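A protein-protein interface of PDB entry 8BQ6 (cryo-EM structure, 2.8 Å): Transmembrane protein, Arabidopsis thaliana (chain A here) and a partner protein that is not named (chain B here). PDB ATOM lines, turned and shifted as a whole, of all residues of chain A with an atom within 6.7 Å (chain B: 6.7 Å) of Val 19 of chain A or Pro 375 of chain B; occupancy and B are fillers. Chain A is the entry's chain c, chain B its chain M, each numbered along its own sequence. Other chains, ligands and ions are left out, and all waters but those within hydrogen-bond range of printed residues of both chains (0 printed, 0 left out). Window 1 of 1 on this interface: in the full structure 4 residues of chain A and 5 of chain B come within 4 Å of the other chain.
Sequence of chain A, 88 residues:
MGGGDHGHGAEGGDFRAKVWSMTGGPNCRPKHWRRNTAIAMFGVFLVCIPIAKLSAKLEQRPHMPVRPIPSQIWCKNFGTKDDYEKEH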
ATOM      1  N   PHE A  15     -21.128  26.493  -6.963  1.00  0.00           N
ATOM      2  CA  PHE A  15     -21.774  26.601  -8.265  1.00  0.00           C
ATOM      3  C   PHE A  15     -21.129  25.699  -9.307  1.00  0.00           C
ATOM      4  O   PHE A  15     -21.758  25.392 -10.324  1.00  0.00           O
ATOM      5  CB  PHE A  15     -21.779  28.058  -8.745  1.00  0.00           C
ATOM      6  CG  PHE A  15     -20.434  28.577  -9.184  1.00  0.00           C
ATOM      7  CD1 PHE A  15     -19.973  28.359 -10.472  1.00  0.00           C
ATOM      8  CD2 PHE A  15     -19.654  29.325  -8.322  1.00  0.00           C
ATOM      9  CE1 PHE A  15     -18.751  28.845 -10.877  1.00  0.00           C
ATOM     10  CE2 PHE A  15     -18.432  29.818  -8.725  1.00  0.00           C
ATOM     11  CZ  PHE A  15     -17.982  29.577 -10.005  1.00  0.00           C
ATOM     12  N   ARG A  16     -19.887  25.269  -9.082  1.00  0.00           N
ATOM     13  CA  ARG A  16     -19.219  24.437 -10.072  1.00  0.00           C
ATOM     14  C   ARG A  16     -19.836  23.049 -10.171  1.00  0.00           C
ATOM     15  O   ARG A  16     -19.595  22.347 -11.156  1.00  0.00           O
ATOM     16  CB  ARG A  16     -17.731  24.355  -9.752  1.00  0.00           C
ATOM     17  CG  ARG A  16     -17.153  25.705  -9.379  1.00  0.00           C
ATOM     18  CD  ARG A  16     -15.796  25.917 -10.004  1.00  0.00           C
ATOM     19  NE  ARG A  16     -14.774  25.130  -9.330  1.00  0.00           N
ATOM     20  CZ  ARG A  16     -14.005  25.583  -8.352  1.00  0.00           C
ATOM     21  NH1 ARG A  16     -14.074  26.837  -7.944  1.00  0.00           N
ATOM     22  NH2 ARG A  16     -13.139  24.757  -7.772  1.00  0.00           N
ATOM     23  N   ALA A  17     -20.642  22.650  -9.188  1.00  0.00           N
ATOM     24  CA  ALA A  17     -21.361  21.388  -9.268  1.00  0.00           C
ATOM     25  C   ALA A  17     -22.492  21.417 -10.289  1.00  0.00           C
ATOM     26  O   ALA A  17     -23.011  20.353 -10.639  1.00  0.00           O
ATOM     27  CB  ALA A  17     -21.915  21.017  -7.894  1.00  0.00           C
ATOM     28  N   LYS A  18     -22.891  22.597 -10.757  1.00  0.00           N
ATOM     29  CA  LYS A  18     -23.915  22.736 -11.783  1.00  0.00           C
ATOM     30  C   LYS A  18     -23.335  23.033 -13.155  1.00  0.00           C
ATOM     31  O   LYS A  18     -24.088  23.356 -14.078  1.00  0.00           O
ATOM     32  CB  LYS A  18     -24.897  23.840 -11.404  1.00  0.00           C
ATOM     33  CG  LYS A  18     -25.396  23.770  -9.983  1.00  0.00           C
ATOM     34  CD  LYS A  18     -26.289  24.955  -9.666  1.00  0.00           C
ATOM     35  CE  LYS A  18     -27.138  25.353 -10.865  1.00  0.00           C
ATOM     36  NZ  LYS A  18     -28.091  24.284 -11.259  1.00  0.00           N
ATOM     37  N   VAL A  19     -22.020  22.944 -13.308  1.00  0.00           N
ATOM     38  CA  VAL A  19     -21.345  23.324 -14.539  1.00  0.00           C
ATOM     39  C   VAL A  19     -20.799  22.061 -15.186  1.00  0.00           C
ATOM     40  O   VAL A  19     -20.005  21.333 -14.579  1.00  0.00           O
ATOM     41  CB  VAL A  19     -20.229  24.345 -14.273  1.00  0.00           C
ATOM     42  CG1 VAL A  19     -19.299  24.438 -15.461  1.00  0.00           C
ATOM     43  CG2 VAL A  19     -20.831  25.702 -13.946  1.00  0.00           C
ATOM     44  N   TRP A  20     -21.232  21.801 -16.415  1.00  0.00           N
ATOM     45  CA  TRP A  20     -20.776  20.651 -17.179  1.00  0.00           C
ATOM     46  C   TRP A  20     -19.482  20.994 -17.909  1.00  0.00           C
ATOM     47  O   TRP A  20     -19.346  22.092 -18.458  1.00  0.00           O
ATOM     48  CB  TRP A  20     -21.853  20.220 -18.173  1.00  0.00           C
ATOM     49  CG  TRP A  20     -21.611  18.883 -18.773  1.00  0.00           C
ATOM     50  CD1 TRP A  20     -22.111  17.700 -18.339  1.00  0.00           C
ATOM     51  CD2 TRP A  20     -20.823  18.586 -19.931  1.00  0.00           C
ATOM     52  NE1 TRP A  20     -21.672  16.675 -19.139  1.00  0.00           N
ATOM     53  CE2 TRP A  20     -20.883  17.195 -20.130  1.00  0.00           C
ATOM     54  CE3 TRP A  20     -20.068  19.360 -20.816  1.00  0.00           C
ATOM     55  CZ2 TRP A  20     -20.218  16.561 -21.174  1.00  0.00           C
ATOM     56  CZ3 TRP A  20     -19.411  18.729 -21.853  1.00  0.00           C
ATOM     57  CH2 TRP A  20     -19.489  17.343 -22.023  1.00  0.00           C
ATOM     58  N   SER A  21     -18.539  20.055 -17.910  1.00  0.00           N
ATOM     59  CA  SER A  21     -17.285  20.214 -18.634  1.00  0.00           C
ATOM     60  C   SER A  21     -16.779  18.846 -19.069  1.00  0.00           C
ATOM     61  O   SER A  21     -17.047  17.828 -18.428  1.00  0.00           O
ATOM     62  CB  SER A  21     -16.220  20.919 -17.787  1.00  0.00           C
ATOM     63  OG  SER A  21     -16.033  20.253 -16.553  1.00  0.00           O
ATOM     64  N   MET A  22     -16.019  18.842 -20.166  1.00  0.00           N
ATOM     65  CA  MET A  22     -15.532  17.585 -20.726  1.00  0.00           C
ATOM     66  C   MET A  22     -14.505  16.920 -19.816  1.00  0.00           C
ATOM     67  O   MET A  22     -14.488  15.690 -19.693  1.00  0.00           O
ATOM     68  CB  MET A  22     -14.944  17.824 -22.117  1.00  0.00           C
ATOM     69  CG  MET A  22     -15.989  17.958 -23.215  1.00  0.00           C
ATOM     70  SD  MET A  22     -15.275  18.231 -24.846  1.00  0.00           S
ATOM     71  CE  MET A  22     -13.832  19.190 -24.415  1.00  0.00           C
ATOM     72  N   GLY A  24     -14.337  17.284 -16.553  1.00  0.00           N
ATOM     73  CA  GLY A  24     -14.956  16.897 -15.306  1.00  0.00           C
ATOM     74  C   GLY A  24     -14.968  17.949 -14.219  1.00  0.00           C
ATOM     75  O   GLY A  24     -15.601  17.726 -13.180  1.00  0.00           O
ATOM     76  N   GLY A  25     -14.301  19.080 -14.416  1.00  0.00           N
ATOM     77  CA  GLY A  25     -14.287  20.120 -13.416  1.00  0.00           C
ATOM     78  C   GLY A  25     -13.405  19.760 -12.239  1.00  0.00           C
ATOM     79  O   GLY A  25     -12.523  18.904 -12.333  1.00  0.00           O
ATOM     80  N   PRO A  26     -13.640  20.398 -11.097  1.00  0.00           N
ATOM     81  CA  PRO A  26     -12.731  20.233  -9.958  1.00  0.00           C
ATOM     82  C   PRO A  26     -13.102  19.052  -9.074  1.00  0.00           C
ATOM     83  O   PRO A  26     -14.267  18.854  -8.718  1.00  0.00           O
ATOM     84  CB  PRO A  26     -12.883  21.555  -9.201  1.00  0.00           C
ATOM     85  CG  PRO A  26     -14.235  22.075  -9.600  1.00  0.00           C
ATOM     86  CD  PRO A  26     -14.752  21.303 -10.778  1.00  0.00           C
ATOM     87  N   LEU B 370     -14.573  33.562 -17.294  1.00  0.00           N
ATOM     88  CA  LEU B 370     -15.649  32.792 -17.902  1.00  0.00           C
ATOM     89  C   LEU B 370     -15.348  31.304 -18.001  1.00  0.00           C
ATOM     90  O   LEU B 370     -16.274  30.526 -18.254  1.00  0.00           O
ATOM     91  CB  LEU B 370     -15.948  33.339 -19.294  1.00  0.00           C
ATOM     92  CG  LEU B 370     -16.730  34.649 -19.339  1.00  0.00           C
ATOM     93  CD1 LEU B 370     -17.010  35.032 -20.775  1.00  0.00           C
ATOM     94  CD2 LEU B 370     -18.017  34.526 -18.556  1.00  0.00           C
ATOM     95  N   VAL B 371     -14.090  30.887 -17.836  1.00  0.00           N
ATOM     96  CA  VAL B 371     -13.779  29.467 -17.956  1.00  0.00           C
ATOM     97  C   VAL B 371     -14.436  28.675 -16.835  1.00  0.00           C
ATOM     98  O   VAL B 371     -14.730  27.484 -16.992  1.00  0.00           O
ATOM     99  CB  VAL B 371     -12.252  29.239 -17.993  1.00  0.00           C
ATOM    100  CG1 VAL B 371     -11.598  29.641 -16.678  1.00  0.00           C
ATOM    101  CG2 VAL B 371     -11.940  27.794 -18.341  1.00  0.00           C
ATOM    102  N   SER B 372     -14.698  29.317 -15.696  1.00  0.00           N
ATOM    103  CA  SER B 372     -15.289  28.613 -14.568  1.00  0.00           C
ATOM    104  C   SER B 372     -16.799  28.441 -14.686  1.00  0.00           C
ATOM    105  O   SER B 372     -17.368  27.616 -13.966  1.00  0.00           O
ATOM    106  CB  SER B 372     -14.949  29.338 -13.266  1.00  0.00           C
ATOM    107  OG  SER B 372     -15.699  30.530 -13.132  1.00  0.00           O
ATOM    108  N   THR B 373     -17.462  29.180 -15.578  1.00  0.00           N
ATOM    109  CA  THR B 373     -18.903  29.052 -15.735  1.00  0.00           C
ATOM    110  C   THR B 373     -19.323  28.556 -17.107  1.00  0.00           C
ATOM    111  O   THR B 373     -20.402  27.968 -17.229  1.00  0.00           O
ATOM    112  CB  THR B 373     -19.599  30.394 -15.468  1.00  0.00           C
ATOM    113  OG1 THR B 373     -18.985  31.421 -16.255  1.00  0.00           O
ATOM    114  CG2 THR B 373     -19.474  30.760 -14.004  1.00  0.00           C
ATOM    115  N   MET B 374     -18.513  28.788 -18.136  1.00  0.00           N
ATOM    116  CA  MET B 374     -18.817  28.359 -19.501  1.00  0.00           C
ATOM    117  C   MET B 374     -17.603  27.667 -20.109  1.00  0.00           C
ATOM    118  O   MET B 374     -17.012  28.157 -21.074  1.00  0.00           O
ATOM    119  CB  MET B 374     -19.246  29.555 -20.350  1.00  0.00           C
ATOM    120  CG  MET B 374     -20.017  30.617 -19.589  1.00  0.00           C
ATOM    121  SD  MET B 374     -20.143  32.183 -20.468  1.00  0.00           S
ATOM    122  CE  MET B 374     -20.988  31.677 -21.958  1.00  0.00           C
ATOM    123  N   PRO B 375     -17.200  26.516 -19.561  1.00  0.00           N
ATOM    124  CA  PRO B 375     -16.025  25.823 -20.114  1.00  0.00           C
ATOM    125  C   PRO B 375     -16.194  25.392 -21.560  1.00  0.00           C
ATOM    126  O   PRO B 375     -15.203  25.355 -22.299  1.00  0.00           O
ATOM    127  CB  PRO B 375     -15.857  24.616 -19.184  1.00  0.00           C
ATOM    128  CG  PRO B 375     -17.188  24.422 -18.564  1.00  0.00           C
ATOM    129  CD  PRO B 375     -17.809  25.767 -18.449  1.00  0.00           C
ATOM    130  N   ASN B 376     -17.413  25.045 -21.984  1.00  0.00           N
ATOM    131  CA  ASN B 376     -17.626  24.638 -23.370  1.00  0.00           C
ATOM    132  C   ASN B 376     -17.376  25.792 -24.328  1.00  0.00           C
ATOM    133  O   ASN B 376     -16.706  25.628 -25.354  1.00  0.00           O
ATOM    134  CB  ASN B 376     -19.042  24.101 -23.556  1.00  0.00           C
ATOM    135  CG  ASN B 376     -19.170  22.663 -23.141  1.00  0.00           C
ATOM    136  OD1 ASN B 376     -18.189  21.926 -23.121  1.00  0.00           O
ATOM    137  ND2 ASN B 376     -20.385  22.247 -22.818  1.00  0.00           N
ATOM    138  N   PHE B 377     -17.927  26.965 -24.017  1.00  0.00           N
ATOM    139  CA  PHE B 377     -17.673  28.144 -24.834  1.00  0.00           C
ATOM    140  C   PHE B 377     -16.198  28.516 -24.805  1.00  0.00           C
ATOM    141  O   PHE B 377     -15.625  28.900 -25.831  1.00  0.00           O
ATOM    142  CB  PHE B 377     -18.547  29.303 -24.348  1.00  0.00           C
ATOM    143  CG  PHE B 377     -18.100  30.656 -24.824  1.00  0.00           C
ATOM    144  CD1 PHE B 377     -18.485  31.131 -26.063  1.00  0.00           C
ATOM    145  CD2 PHE B 377     -17.317  31.464 -24.019  1.00  0.00           C
ATOM    146  CE1 PHE B 377     -18.082  32.373 -26.500  1.00  0.00           C
ATOM    147  CE2 PHE B 377     -16.911  32.706 -24.452  1.00  0.00           C
ATOM    148  CZ  PHE B 377     -17.299  33.163 -25.693  1.00  0.00           C
ATOM    149  N   SER B 378     -15.562  28.392 -23.640  1.00  0.00           N
ATOM    150  CA  SER B 378     -14.155  28.757 -23.517  1.00  0.00           C
ATOM    151  C   SER B 378     -13.269  27.882 -24.397  1.00  0.00           C
ATOM    152  O   SER B 378     -12.296  28.368 -24.986  1.00  0.00           O
ATOM    153  CB  SER B 378     -13.724  28.671 -22.056  1.00  0.00           C
ATOM    154  OG  SER B 378     -14.372  29.665 -21.282  1.00  0.00           O
ATOM    155  N   THR B 379     -13.579  26.586 -24.494  1.00  0.00           N
ATOM    156  CA  THR B 379     -12.777  25.697 -25.330  1.00  0.00           C
ATOM    157  C   THR B 379     -12.968  26.013 -26.809  1.00  0.00           C
ATOM    158  O   THR B 379     -11.997  26.071 -27.573  1.00  0.00           O
ATOM    159  CB  THR B 379     -13.136  24.239 -25.046  1.00  0.00           C
ATOM    160  OG1 THR B 379     -12.868  23.944 -23.672  1.00  0.00           O
ATOM    161  CG2 THR B 379     -12.297  23.313 -25.911  1.00  0.00           C
ATOM    162  N   ILE B 380     -14.218  26.211 -27.229  1.00  0.00           N
ATOM    163  CA  ILE B 380     -14.508  26.568 -28.615  1.00  0.00           C
ATOM    164  C   ILE B 380     -13.914  27.929 -28.950  1.00  0.00           C
ATOM    165  O   ILE B 380     -13.386  28.144 -30.048  1.00  0.00           O
ATOM    166  CB  ILE B 380     -16.030  26.530 -28.856  1.00  0.00           C
ATOM    167  CG1 ILE B 380     -16.519  25.081 -28.903  1.00  0.00           C
ATOM    168  CG2 ILE B 380     -16.415  27.281 -30.118  1.00  0.00           C
ATOM    169  CD1 ILE B 380     -18.009  24.942 -28.988  1.00  0.00           C
ATOM    170  N   ASP B 451     -23.881  28.278 -20.222  1.00  0.00           N
ATOM    171  CA  ASP B 451     -23.018  27.814 -21.292  1.00  0.00           C
ATOM    172  C   ASP B 451     -23.834  27.618 -22.566  1.00  0.00           C
ATOM    173  O   ASP B 451     -25.040  27.874 -22.615  1.00  0.00           O
ATOM    174  CB  ASP B 451     -22.316  26.523 -20.885  1.00  0.00           C
ATOM    175  CG  ASP B 451     -20.926  26.409 -21.467  1.00  0.00           C
ATOM    176  OD1 ASP B 451     -20.640  27.099 -22.465  1.00  0.00           O
ATOM    177  OD2 ASP B 451     -20.115  25.635 -20.923  1.00  0.00           O
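The backbone NH of Gly 25 of chain A lies within hydrogen-bond range of the side-chain hydroxyl of Ser 21 of chain A, at 3.0 Å.
N of Gly 24 of chain A lies within hydrogen-bond range of OG of Ser 21 of chain A, 3.4 Å away.
The backbone carbonyl oxygen (O) of Leu 370 of chain B is in hydrogen-bond range of the side-chain hydroxyl (OG1) of Thr 373 of chain B, at 3.5 Å.
The backbone NH (N) of Asn 376 of chain B lies within hydrogen-bond range of the side-chain carboxylate (OD2) of Asp 451 of chain B, 3.0 Å away.
The backbone carbonyl oxygen of Pro 375 of chain B is in hydrogen-bond range of the side-chain hydroxyl of Thr 379 of chain B (3.1 Å).
Phe 15 of chain A touches Ser 372 of chain B.
Phe 15 of chain A touches Thr 373 of chain B (CE1 to CG2, 3.7 Å).
Val 19 of chain A touches Ser 372 of chain B.
Pro 375 of chain B touches Val 19 of chain A (CD to CG1, 3.6 Å).
O of Trp 20 of chain A touches CG of Pro 375 of chain B (3.2 Å).
CE3 of Trp 20 of chain A touches ND2 of Asn 376 of chain B (3.5 Å).
CB of Ser 21 of chain A touches CG of Pro 375 of chain B (3.7 Å).
Of the printed residues of chain B, Val 19 of chain A touches Ser 372 and Pro 375.
Of chain A, only Val 19 (3.6 Å), Trp 20 (3.2 Å) and Ser 21 (3.7 Å) come within 4 Å of Pro 375 of chain B.
Of the printed residues of chain A, Ser 372 of chain B touches Phe 15 (3.6 Å) and Val 19 (3.96 Å).
Printed residues of chain B within 4 Å of Phe 15 of chain A: Ser 372 (3.6 Å) and Thr 373 (3.7 Å).
Of the printed residues of chain B, Trp 20 of chain A touches Pro 375 (3.2 Å) and Asn 376 (3.5 Å).
Met 374 of chain B touches none of the printed residues of chain A.
Pro 26 of chain A touches none of the printed residues of chain B.
The nearest residue of chain A that does not touch Pro 375 of chain B is Met 22 of chain A (5.9 Å).
Of the 11 printed residues of chain A, 4 touch a printed residue of chain B.
Printed residues of chain A that touch a printed residue of chain B: Phe 15, Val 19, Trp 20 and Ser 21.
Among the printed residues, 7 pairs touch across the chains.
Among the printed residues, no Asp or Glu carboxylate lies within 4 Å of a Lys or Arg side-chain nitrogen of the other chain.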
